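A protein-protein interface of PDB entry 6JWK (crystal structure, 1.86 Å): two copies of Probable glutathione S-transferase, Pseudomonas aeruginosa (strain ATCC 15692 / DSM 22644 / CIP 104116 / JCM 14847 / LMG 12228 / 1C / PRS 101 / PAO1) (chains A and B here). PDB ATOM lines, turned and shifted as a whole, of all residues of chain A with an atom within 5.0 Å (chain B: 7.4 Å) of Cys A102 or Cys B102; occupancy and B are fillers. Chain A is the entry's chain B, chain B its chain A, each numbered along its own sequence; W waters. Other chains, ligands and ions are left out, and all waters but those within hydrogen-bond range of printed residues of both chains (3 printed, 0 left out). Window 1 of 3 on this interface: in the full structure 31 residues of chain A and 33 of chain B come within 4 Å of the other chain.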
ATOM      1  N   GLN A  65      15.768 -16.625  -4.331  1.00  0.00           N
ATOM      2  CA  GLN A  65      14.393 -16.985  -3.919  1.00  0.00           C
ATOM      3  C   GLN A  65      13.514 -16.901  -5.160  1.00  0.00           C
ATOM      4  O   GLN A  65      13.121 -15.812  -5.594  1.00  0.00           O
ATOM      5  CB  GLN A  65      13.884 -16.222  -2.708  1.00  0.00           C
ATOM      6  CG  GLN A  65      14.636 -16.555  -1.414  1.00  0.00           C
ATOM      7  CD  GLN A  65      14.484 -17.996  -0.989  1.00  0.00           C
ATOM      8  OE1 GLN A  65      13.460 -18.651  -1.247  1.00  0.00           O
ATOM      9  NE2 GLN A  65      15.524 -18.516  -0.347  1.00  0.00           N
ATOM     10  N   ALA A  97       0.590 -21.435  -4.293  1.00  0.00           N
ATOM     11  CA  ALA A  97       2.043 -21.377  -4.614  1.00  0.00           C
ATOM     12  C   ALA A  97       2.887 -21.672  -3.361  1.00  0.00           C
ATOM     13  O   ALA A  97       3.872 -22.415  -3.482  1.00  0.00           O
ATOM     14  CB  ALA A  97       2.403 -20.045  -5.245  1.00  0.00           C
ATOM     15  N   LEU A  98       2.507 -21.117  -2.208  1.00  0.00           N
ATOM     16  CA  LEU A  98       3.259 -21.215  -0.932  1.00  0.00           C
ATOM     17  C   LEU A  98       3.020 -22.584  -0.341  1.00  0.00           C
ATOM     18  O   LEU A  98       3.966 -23.108   0.250  1.00  0.00           O
ATOM     19  CB  LEU A  98       2.846 -20.107   0.041  1.00  0.00           C
ATOM     20  CG  LEU A  98       3.342 -18.747  -0.415  1.00  0.00           C
ATOM     21  CD1 LEU A  98       2.527 -17.665   0.270  1.00  0.00           C
ATOM     22  CD2 LEU A  98       4.838 -18.588  -0.130  1.00  0.00           C
ATOM     23  N   LEU A  99       1.870 -23.198  -0.595  1.00  0.00           N
ATOM     24  CA  LEU A  99       1.691 -24.615  -0.187  1.00  0.00           C
ATOM     25  C   LEU A  99       2.776 -25.491  -0.806  1.00  0.00           C
ATOM     26  O   LEU A  99       3.385 -26.326  -0.096  1.00  0.00           O
ATOM     27  CB  LEU A  99       0.296 -25.083  -0.588  1.00  0.00           C
ATOM     28  CG  LEU A  99      -0.028 -26.554  -0.380  1.00  0.00           C
ATOM     29  CD1 LEU A  99      -0.019 -26.932   1.108  1.00  0.00           C
ATOM     30  CD2 LEU A  99      -1.419 -26.794  -0.949  1.00  0.00           C
ATOM     31  N   VAL A 100       2.991 -25.370  -2.107  1.00  0.00           N
ATOM     32  CA  VAL A 100       4.074 -26.106  -2.802  1.00  0.00           C
ATOM     33  C   VAL A 100       5.454 -25.653  -2.281  1.00  0.00           C
ATOM     34  O   VAL A 100       6.247 -26.527  -1.886  1.00  0.00           O
ATOM     35  CB  VAL A 100       3.959 -25.901  -4.312  1.00  0.00           C
ATOM     36  CG1 VAL A 100       5.107 -26.594  -5.020  1.00  0.00           C
ATOM     37  CG2 VAL A 100       2.586 -26.426  -4.759  1.00  0.00           C
ATOM     38  N   ALA A 101       5.710 -24.349  -2.246  1.00  0.00           N
ATOM     39  CA  ALA A 101       7.065 -23.789  -2.042  1.00  0.00           C
ATOM     40  C   ALA A 101       7.502 -23.894  -0.571  1.00  0.00           C
ATOM     41  O   ALA A 101       8.691 -23.834  -0.328  1.00  0.00           O
ATOM     42  CB  ALA A 101       7.121 -22.373  -2.586  1.00  0.00           C
ATOM     43  N   CYS A 102       6.573 -23.961   0.370  1.00  0.00           N
ATOM     44  CA  CYS A 102       6.831 -24.005   1.839  1.00  0.00           C
ATOM     45  C   CYS A 102       6.557 -25.397   2.423  1.00  0.00           C
ATOM     46  O   CYS A 102       7.311 -25.792   3.295  1.00  0.00           O
ATOM     47  CB  CYS A 102       5.972 -23.015   2.618  1.00  0.00           C
ATOM     48  SG  CYS A 102       6.302 -21.317   2.132  1.00  0.00           S
ATOM     49  N   ASP A 103       5.521 -26.106   1.963  1.00  0.00           N
ATOM     50  CA  ASP A 103       4.988 -27.306   2.668  1.00  0.00           C
ATOM     51  C   ASP A 103       5.310 -28.588   1.920  1.00  0.00           C
ATOM     52  O   ASP A 103       5.072 -29.656   2.511  1.00  0.00           O
ATOM     53  CB  ASP A 103       3.488 -27.199   2.923  1.00  0.00           C
ATOM     54  CG  ASP A 103       3.141 -26.053   3.881  1.00  0.00           C
ATOM     55  OD1 ASP A 103       4.093 -25.487   4.479  1.00  0.00           O
ATOM     56  OD2 ASP A 103       1.955 -25.698   3.975  1.00  0.00           O
ATOM     57  N   ILE A 104       5.777 -28.527   0.669  1.00  0.00           N
ATOM     58  CA  ILE A 104       6.153 -29.782  -0.062  1.00  0.00           C
ATOM     59  C   ILE A 104       7.635 -29.767  -0.426  1.00  0.00           C
ATOM     60  O   ILE A 104       8.410 -30.607   0.140  1.00  0.00           O
ATOM     61  CB  ILE A 104       5.301 -30.011  -1.324  1.00  0.00           C
ATOM     62  CG1 ILE A 104       3.807 -29.896  -1.047  1.00  0.00           C
ATOM     63  CG2 ILE A 104       5.680 -31.342  -1.928  1.00  0.00           C
ATOM     64  CD1 ILE A 104       2.946 -30.040  -2.287  1.00  0.00           C
ATOM     65  N   PRO A 106      10.461 -28.012   0.061  1.00  0.00           N
ATOM     66  CA  PRO A 106      11.626 -27.934   0.957  1.00  0.00           C
ATOM     67  C   PRO A 106      11.996 -29.260   1.657  1.00  0.00           C
ATOM     68  O   PRO A 106      13.168 -29.458   1.956  1.00  0.00           O
ATOM     69  CB  PRO A 106      11.215 -26.916   2.009  1.00  0.00           C
ATOM     70  CG  PRO A 106      10.198 -26.050   1.287  1.00  0.00           C
ATOM     71  CD  PRO A 106       9.412 -27.060   0.436  1.00  0.00           C
ATOM     72  N   ARG B  14       3.770 -15.507  13.340  1.00  0.00           N
ATOM     73  CA  ARG B  14       3.982 -14.601  12.185  1.00  0.00           C
ATOM     74  C   ARG B  14       2.740 -13.751  11.963  1.00  0.00           C
ATOM     75  O   ARG B  14       2.821 -12.527  11.834  1.00  0.00           O
ATOM     76  CB  ARG B  14       4.241 -15.369  10.891  1.00  0.00           C
ATOM     77  CG  ARG B  14       5.605 -16.037  10.813  1.00  0.00           C
ATOM     78  CD  ARG B  14       5.718 -16.791   9.498  1.00  0.00           C
ATOM     79  NE  ARG B  14       6.797 -17.725   9.522  1.00  0.00           N
ATOM     80  CZ  ARG B  14       6.966 -18.705   8.667  1.00  0.00           C
ATOM     81  NH1 ARG B  14       6.120 -18.856   7.666  1.00  0.00           N
ATOM     82  NH2 ARG B  14       8.024 -19.494   8.759  1.00  0.00           N
ATOM     83  N   GLN B  65      -1.793 -19.984   4.674  1.00  0.00           N
ATOM     84  CA  GLN B  65      -0.355 -19.725   4.394  1.00  0.00           C
ATOM     85  C   GLN B  65      -0.001 -18.320   4.926  1.00  0.00           C
ATOM     86  O   GLN B  65      -0.480 -17.287   4.406  1.00  0.00           O
ATOM     87  CB  GLN B  65      -0.075 -19.884   2.911  1.00  0.00           C
ATOM     88  CG  GLN B  65      -0.223 -21.304   2.405  1.00  0.00           C
ATOM     89  CD  GLN B  65       0.872 -22.205   2.902  1.00  0.00           C
ATOM     90  OE1 GLN B  65       1.999 -21.759   3.194  1.00  0.00           O
ATOM     91  NE2 GLN B  65       0.509 -23.467   3.016  1.00  0.00           N
ATOM     92  N   SER B  66       0.831 -18.283   5.962  1.00  0.00           N
ATOM     93  CA  SER B  66       1.170 -17.049   6.700  1.00  0.00           C
ATOM     94  C   SER B  66       1.598 -15.961   5.736  1.00  0.00           C
ATOM     95  O   SER B  66       1.156 -14.800   5.946  1.00  0.00           O
ATOM     96  CB  SER B  66       2.235 -17.337   7.764  1.00  0.00           C
ATOM     97  OG  SER B  66       3.342 -18.050   7.241  1.00  0.00           O
ATOM     98  N   LEU B  67       2.451 -16.245   4.731  1.00  0.00           N
ATOM     99  CA  LEU B  67       2.960 -15.133   3.890  1.00  0.00           C
ATOM    100  C   LEU B  67       1.858 -14.619   2.949  1.00  0.00           C
ATOM    101  O   LEU B  67       1.857 -13.434   2.657  1.00  0.00           O
ATOM    102  CB  LEU B  67       4.215 -15.462   3.070  1.00  0.00           C
ATOM    103  CG  LEU B  67       5.451 -16.024   3.761  1.00  0.00           C
ATOM    104  CD1 LEU B  67       6.659 -15.698   2.920  1.00  0.00           C
ATOM    105  CD2 LEU B  67       5.669 -15.569   5.143  1.00  0.00           C
ATOM    106  N   LEU B  96      14.328 -12.310   1.967  1.00  0.00           N
ATOM    107  CA  LEU B  96      14.645 -12.703   3.370  1.00  0.00           C
ATOM    108  C   LEU B  96      13.451 -13.433   4.017  1.00  0.00           C
ATOM    109  O   LEU B  96      13.680 -14.477   4.654  1.00  0.00           O
ATOM    110  CB  LEU B  96      15.104 -11.438   4.126  1.00  0.00           C
ATOM    111  CG  LEU B  96      15.531 -11.594   5.579  1.00  0.00           C
ATOM    112  CD1 LEU B  96      16.404 -12.773   5.810  1.00  0.00           C
ATOM    113  CD2 LEU B  96      16.188 -10.322   6.040  1.00  0.00           C
ATOM    114  N   ALA B  97      12.222 -12.981   3.789  1.00  0.00           N
ATOM    115  CA  ALA B  97      11.007 -13.650   4.301  1.00  0.00           C
ATOM    116  C   ALA B  97      10.933 -15.089   3.761  1.00  0.00           C
ATOM    117  O   ALA B  97      10.662 -16.033   4.572  1.00  0.00           O
ATOM    118  CB  ALA B  97       9.781 -12.854   3.945  1.00  0.00           C
ATOM    119  N   LEU B  98      11.216 -15.298   2.472  1.00  0.00           N
ATOM    120  CA  LEU B  98      11.105 -16.670   1.870  1.00  0.00           C
ATOM    121  C   LEU B  98      12.271 -17.550   2.269  1.00  0.00           C
ATOM    122  O   LEU B  98      12.089 -18.772   2.386  1.00  0.00           O
ATOM    123  CB  LEU B  98      10.996 -16.549   0.352  1.00  0.00           C
ATOM    124  CG  LEU B  98       9.694 -15.941  -0.129  1.00  0.00           C
ATOM    125  CD1 LEU B  98       9.861 -15.415  -1.549  1.00  0.00           C
ATOM    126  CD2 LEU B  98       8.559 -16.965  -0.084  1.00  0.00           C
ATOM    127  N   LEU B  99      13.449 -16.978   2.503  1.00  0.00           N
ATOM    128  CA  LEU B  99      14.572 -17.756   3.074  1.00  0.00           C
ATOM    129  C   LEU B  99      14.057 -18.435   4.339  1.00  0.00           C
ATOM    130  O   LEU B  99      14.220 -19.684   4.502  1.00  0.00           O
ATOM    131  CB  LEU B  99      15.761 -16.833   3.328  1.00  0.00           C
ATOM    132  CG  LEU B  99      16.940 -17.428   4.090  1.00  0.00           C
ATOM    133  CD1 LEU B  99      17.649 -18.514   3.276  1.00  0.00           C
ATOM    134  CD2 LEU B  99      17.920 -16.324   4.442  1.00  0.00           C
ATOM    135  N   VAL B 100      13.424 -17.667   5.202  1.00  0.00           N
ATOM    136  CA  VAL B 100      12.881 -18.205   6.468  1.00  0.00           C
ATOM    137  C   VAL B 100      11.724 -19.158   6.175  1.00  0.00           C
ATOM    138  O   VAL B 100      11.750 -20.293   6.694  1.00  0.00           O
ATOM    139  CB  VAL B 100      12.448 -17.090   7.421  1.00  0.00           C
ATOM    140  CG1 VAL B 100      11.758 -17.671   8.653  1.00  0.00           C
ATOM    141  CG2 VAL B 100      13.645 -16.236   7.821  1.00  0.00           C
ATOM    142  N   ALA B 101      10.747 -18.737   5.384  1.00  0.00           N
ATOM    143  CA  ALA B 101       9.466 -19.487   5.256  1.00  0.00           C
ATOM    144  C   ALA B 101       9.627 -20.770   4.420  1.00  0.00           C
ATOM    145  O   ALA B 101       8.768 -21.661   4.545  1.00  0.00           O
ATOM    146  CB  ALA B 101       8.433 -18.575   4.666  1.00  0.00           C
ATOM    147  N   CYS B 102      10.613 -20.827   3.525  1.00  0.00           N
ATOM    148  CA  CYS B 102      10.825 -21.951   2.587  1.00  0.00           C
ATOM    149  C   CYS B 102      12.069 -22.753   2.957  1.00  0.00           C
ATOM    150  O   CYS B 102      12.039 -23.971   2.727  1.00  0.00           O
ATOM    151  CB  CYS B 102      11.005 -21.475   1.148  1.00  0.00           C
ATOM    152  SG  CYS B 102       9.573 -20.566   0.555  1.00  0.00           S
ATOM    153  N   ASP B 103      13.139 -22.131   3.476  1.00  0.00           N
ATOM    154  CA  ASP B 103      14.434 -22.857   3.574  1.00  0.00           C
ATOM    155  C   ASP B 103      14.818 -23.174   5.028  1.00  0.00           C
ATOM    156  O   ASP B 103      15.849 -23.864   5.215  1.00  0.00           O
ATOM    157  CB  ASP B 103      15.578 -22.132   2.864  1.00  0.00           C
ATOM    158  CG  ASP B 103      15.391 -21.887   1.376  1.00  0.00           C
ATOM    159  OD1 ASP B 103      14.532 -22.545   0.730  1.00  0.00           O
ATOM    160  OD2 ASP B 103      16.091 -21.012   0.855  1.00  0.00           O
ATOM    161  N   ILE B 104      14.110 -22.667   6.037  1.00  0.00           N
ATOM    162  CA  ILE B 104      14.427 -23.003   7.451  1.00  0.00           C
ATOM    163  C   ILE B 104      13.216 -23.696   8.071  1.00  0.00           C
ATOM    164  O   ILE B 104      13.283 -24.918   8.400  1.00  0.00           O
ATOM    165  CB  ILE B 104      14.871 -21.760   8.271  1.00  0.00           C
ATOM    166  CG1 ILE B 104      15.898 -20.917   7.526  1.00  0.00           C
ATOM    167  CG2 ILE B 104      15.360 -22.163   9.645  1.00  0.00           C
ATOM    168  CD1 ILE B 104      16.325 -19.618   8.254  1.00  0.00           C
ATOM    169  N   HIS B 105      12.143 -22.950   8.268  1.00  0.00           N
ATOM    170  CA  HIS B 105      11.037 -23.414   9.132  1.00  0.00           C
ATOM    171  C   HIS B 105      10.491 -24.773   8.684  1.00  0.00           C
ATOM    172  O   HIS B 105      10.195 -25.617   9.548  1.00  0.00           O
ATOM    173  CB  HIS B 105       9.937 -22.379   9.199  1.00  0.00           C
ATOM    174  CG  HIS B 105       8.882 -22.816  10.141  1.00  0.00           C
ATOM    175  ND1 HIS B 105       9.151 -23.044  11.489  1.00  0.00           N
ATOM    176  CD2 HIS B 105       7.583 -23.160   9.924  1.00  0.00           C
ATOM    177  CE1 HIS B 105       8.045 -23.495  12.066  1.00  0.00           C
ATOM    178  NE2 HIS B 105       7.068 -23.538  11.123  1.00  0.00           N
ATOM    179  N   PRO B 106      10.222 -25.005   7.368  1.00  0.00           N
ATOM    180  CA  PRO B 106       9.561 -26.244   6.934  1.00  0.00           C
ATOM    181  C   PRO B 106      10.282 -27.510   7.383  1.00  0.00           C
ATOM    182  O   PRO B 106       9.612 -28.434   7.706  1.00  0.00           O
ATOM    183  CB  PRO B 106       9.614 -26.154   5.408  1.00  0.00           C
ATOM    184  CG  PRO B 106       9.540 -24.682   5.158  1.00  0.00           C
ATOM    185  CD  PRO B 106      10.446 -24.102   6.234  1.00  0.00           C
ATOM    186  N   LEU B 107      11.622 -27.489   7.397  1.00  0.00           N
ATOM    187  CA  LEU B 107      12.472 -28.625   7.834  1.00  0.00           C
ATOM    188  C   LEU B 107      12.386 -28.857   9.351  1.00  0.00           C
ATOM    189  O   LEU B 107      12.578 -30.003   9.784  1.00  0.00           O
ATOM    190  CB  LEU B 107      13.912 -28.362   7.384  1.00  0.00           C
ATOM    191  CG  LEU B 107      14.066 -28.234   5.870  1.00  0.00           C
ATOM    192  CD1 LEU B 107      15.444 -27.775   5.495  1.00  0.00           C
ATOM    193  CD2 LEU B 107      13.772 -29.561   5.203  1.00  0.00           C
ATOM    194  N   ASN B 109       9.653 -27.962  11.425  1.00  0.00           N
ATOM    195  CA  ASN B 109       8.236 -28.117  11.838  1.00  0.00           C
ATOM    196  C   ASN B 109       8.090 -29.237  12.896  1.00  0.00           C
ATOM    197  O   ASN B 109       8.808 -30.258  12.806  1.00  0.00           O
ATOM    198  CB  ASN B 109       7.426 -28.514  10.598  1.00  0.00           C
ATOM    199  CG  ASN B 109       6.084 -27.842  10.507  1.00  0.00           C
ATOM    200  OD1 ASN B 109       5.186 -28.112  11.314  1.00  0.00           O
ATOM    201  ND2 ASN B 109       5.936 -27.007   9.488  1.00  0.00           N
ATOM    202  N   ARG B 111       5.603 -31.373  12.712  1.00  0.00           N
ATOM    203  CA  ARG B 111       5.188 -32.561  11.899  1.00  0.00           C
ATOM    204  C   ARG B 111       6.435 -33.295  11.356  1.00  0.00           C
ATOM    205  O   ARG B 111       6.465 -34.526  11.420  1.00  0.00           O
ATOM    206  CB  ARG B 111       4.131 -32.180  10.851  1.00  0.00           C
ATOM    207  CG  ARG B 111       4.685 -31.468   9.627  1.00  0.00           C
ATOM    208  CD  ARG B 111       3.668 -31.141   8.525  1.00  0.00           C
ATOM    209  NE  ARG B 111       4.412 -30.454   7.479  1.00  0.00           N
ATOM    210  CZ  ARG B 111       4.207 -30.533   6.179  1.00  0.00           C
ATOM    211  NH1 ARG B 111       3.220 -31.257   5.661  1.00  0.00           N
ATOM    212  NH2 ARG B 111       5.022 -29.857   5.390  1.00  0.00           N
HETATM  213  O   HOH W   1       3.496 -31.802   2.619  1.00  0.00           O
HETATM  214  O   HOH W   2       3.593 -22.388   5.259  1.00  0.00           O
HETATM  215  O   HOH W   3      13.426 -21.235  -1.687  1.00  0.00           O
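O of Leu B98 sits close to SG of Cys B102 (3.6 Å).
The backbone carbonyl oxygen (O) of Leu B99 is in hydrogen-bond range of the backbone NH (N) of Ile B104 (3.4 Å).
O of Leu A99 sits at hydrogen-bond distance from N of Ile A104 (3.3 Å).
The side-chain sulfur of Cys A102 lies close to the backbone carbonyl oxygen of Leu A98 (3.5 Å).
Gln A65 touches Leu B98, and with the chains exchanged Leu A98 touches Gln B65.
Cys A102 touches its own counterpart, Cys B102.
Cys A102 touches Pro B106, and with the chains exchanged Pro A106 touches Cys B102.
Pro B106 touches its own counterpart, Pro A106.
Of the 15 pairs that touch across the chains among the printed residues, 12 have their exchanged pair printed and touching as well.
OE1 of Gln A65 touches CB of Leu B98, at 3.6 Å.
Gln A65 touches Leu B99 (NE2 to CA, 3.6 Å).
Leu A98 touches Gln B65 (CB to OE1, 3.7 Å).
Leu A98 touches Leu B67 (CD1 to CB, 3.9 Å).
Gln B65 touches Leu A99 (NE2 to CA, 3.6 Å).
O of Cys A102 touches CG of Pro B106 (3.1 Å).
Cys B102 touches Pro A106.
CB of Pro A106 touches CB of Pro B106, at 3.8 Å.
Pro A106 touches Leu B107.
Water W3 lies within hydrogen-bond range of the side-chain amide oxygen of Gln A65 (2.6 Å) and the side-chain carboxylate of Asp B103 (3.0 Å).
Water W1 lies within hydrogen-bond range of the backbone carbonyl oxygen (O) of Asp A103 (2.7 Å) and the guanidinium group (NH1) of Arg B111 (3.1 Å).
Water W2 bridges OE1 of Gln B65 and OD1 of Asp A103.
The side-chain sulfur (SG) of Cys A102 lies within hydrogen-bond range of the backbone carbonyl oxygen (O) of Ala B101, at 3.5 Å.
The side-chain amide nitrogen of Gln B65 lies within hydrogen-bond range of the side-chain carboxylate of Asp A103 (2.8 Å).
The side-chain sulfur of Cys B102 is in hydrogen-bond range of the backbone carbonyl oxygen of Ala A101, 3.5 Å away.
The guanidinium group of Arg B111 lies within hydrogen-bond range of the backbone carbonyl oxygen of Asp A103.
The side-chain sulfur (SG) of Cys B102 sits at hydrogen-bond distance from the side-chain sulfur (SG) of Cys A102.
The side-chain carboxylate (OD2) of Asp B103 is in hydrogen-bond range of the side-chain amide nitrogen (NE2) of Gln A65, at 2.8 Å.
Of chain B, only Ala B101 (3.5 Å), Cys B102 (3.7 Å) and Pro B106 (3.1 Å) come within 4 Å of Cys A102.
Of chain A, only Ala A101, Cys A102 and Pro A106 come within 4 Å of Cys B102.
Printed residues of chain B within 4 Å of Ala A101: Cys B102 (3.5 Å).
Of the printed residues of chain B, Leu A99 touches Gln B65 (3.6 Å).
Printed residues of chain A within 4 Å of Leu B98: Gln A65 (3.6 Å).
Of the printed residues of chain B, Gln A65 touches Leu B98 (3.6 Å), Leu B99 (3.6 Å) and Asp B103 (2.8 Å).
Printed residues of chain A within 4 Å of Leu B107: Pro A106 (3.3 Å).
Val B100 touches none of the printed residues of chain A.
The nearest residue of chain A that does not touch Cys B102 is Gln A65 (4.4 Å).
The nearest printed residue of chain A that does not touch Leu B107 is Cys A102 (6.2 Å).
Hydrophobic or aromatic side chains of chain B within 4 Å of the printed part of chain A: Leu B67, Leu B98, Pro B106 and Leu B107.
Of the 10 printed residues of chain A, 7 touch a printed residue of chain B.
Hydrophobic or aromatic side chains of chain A that line the printed part of chain B: Leu A98, Leu A99 and Pro A106.
Among the printed residues, 15 pairs touch across the chains.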
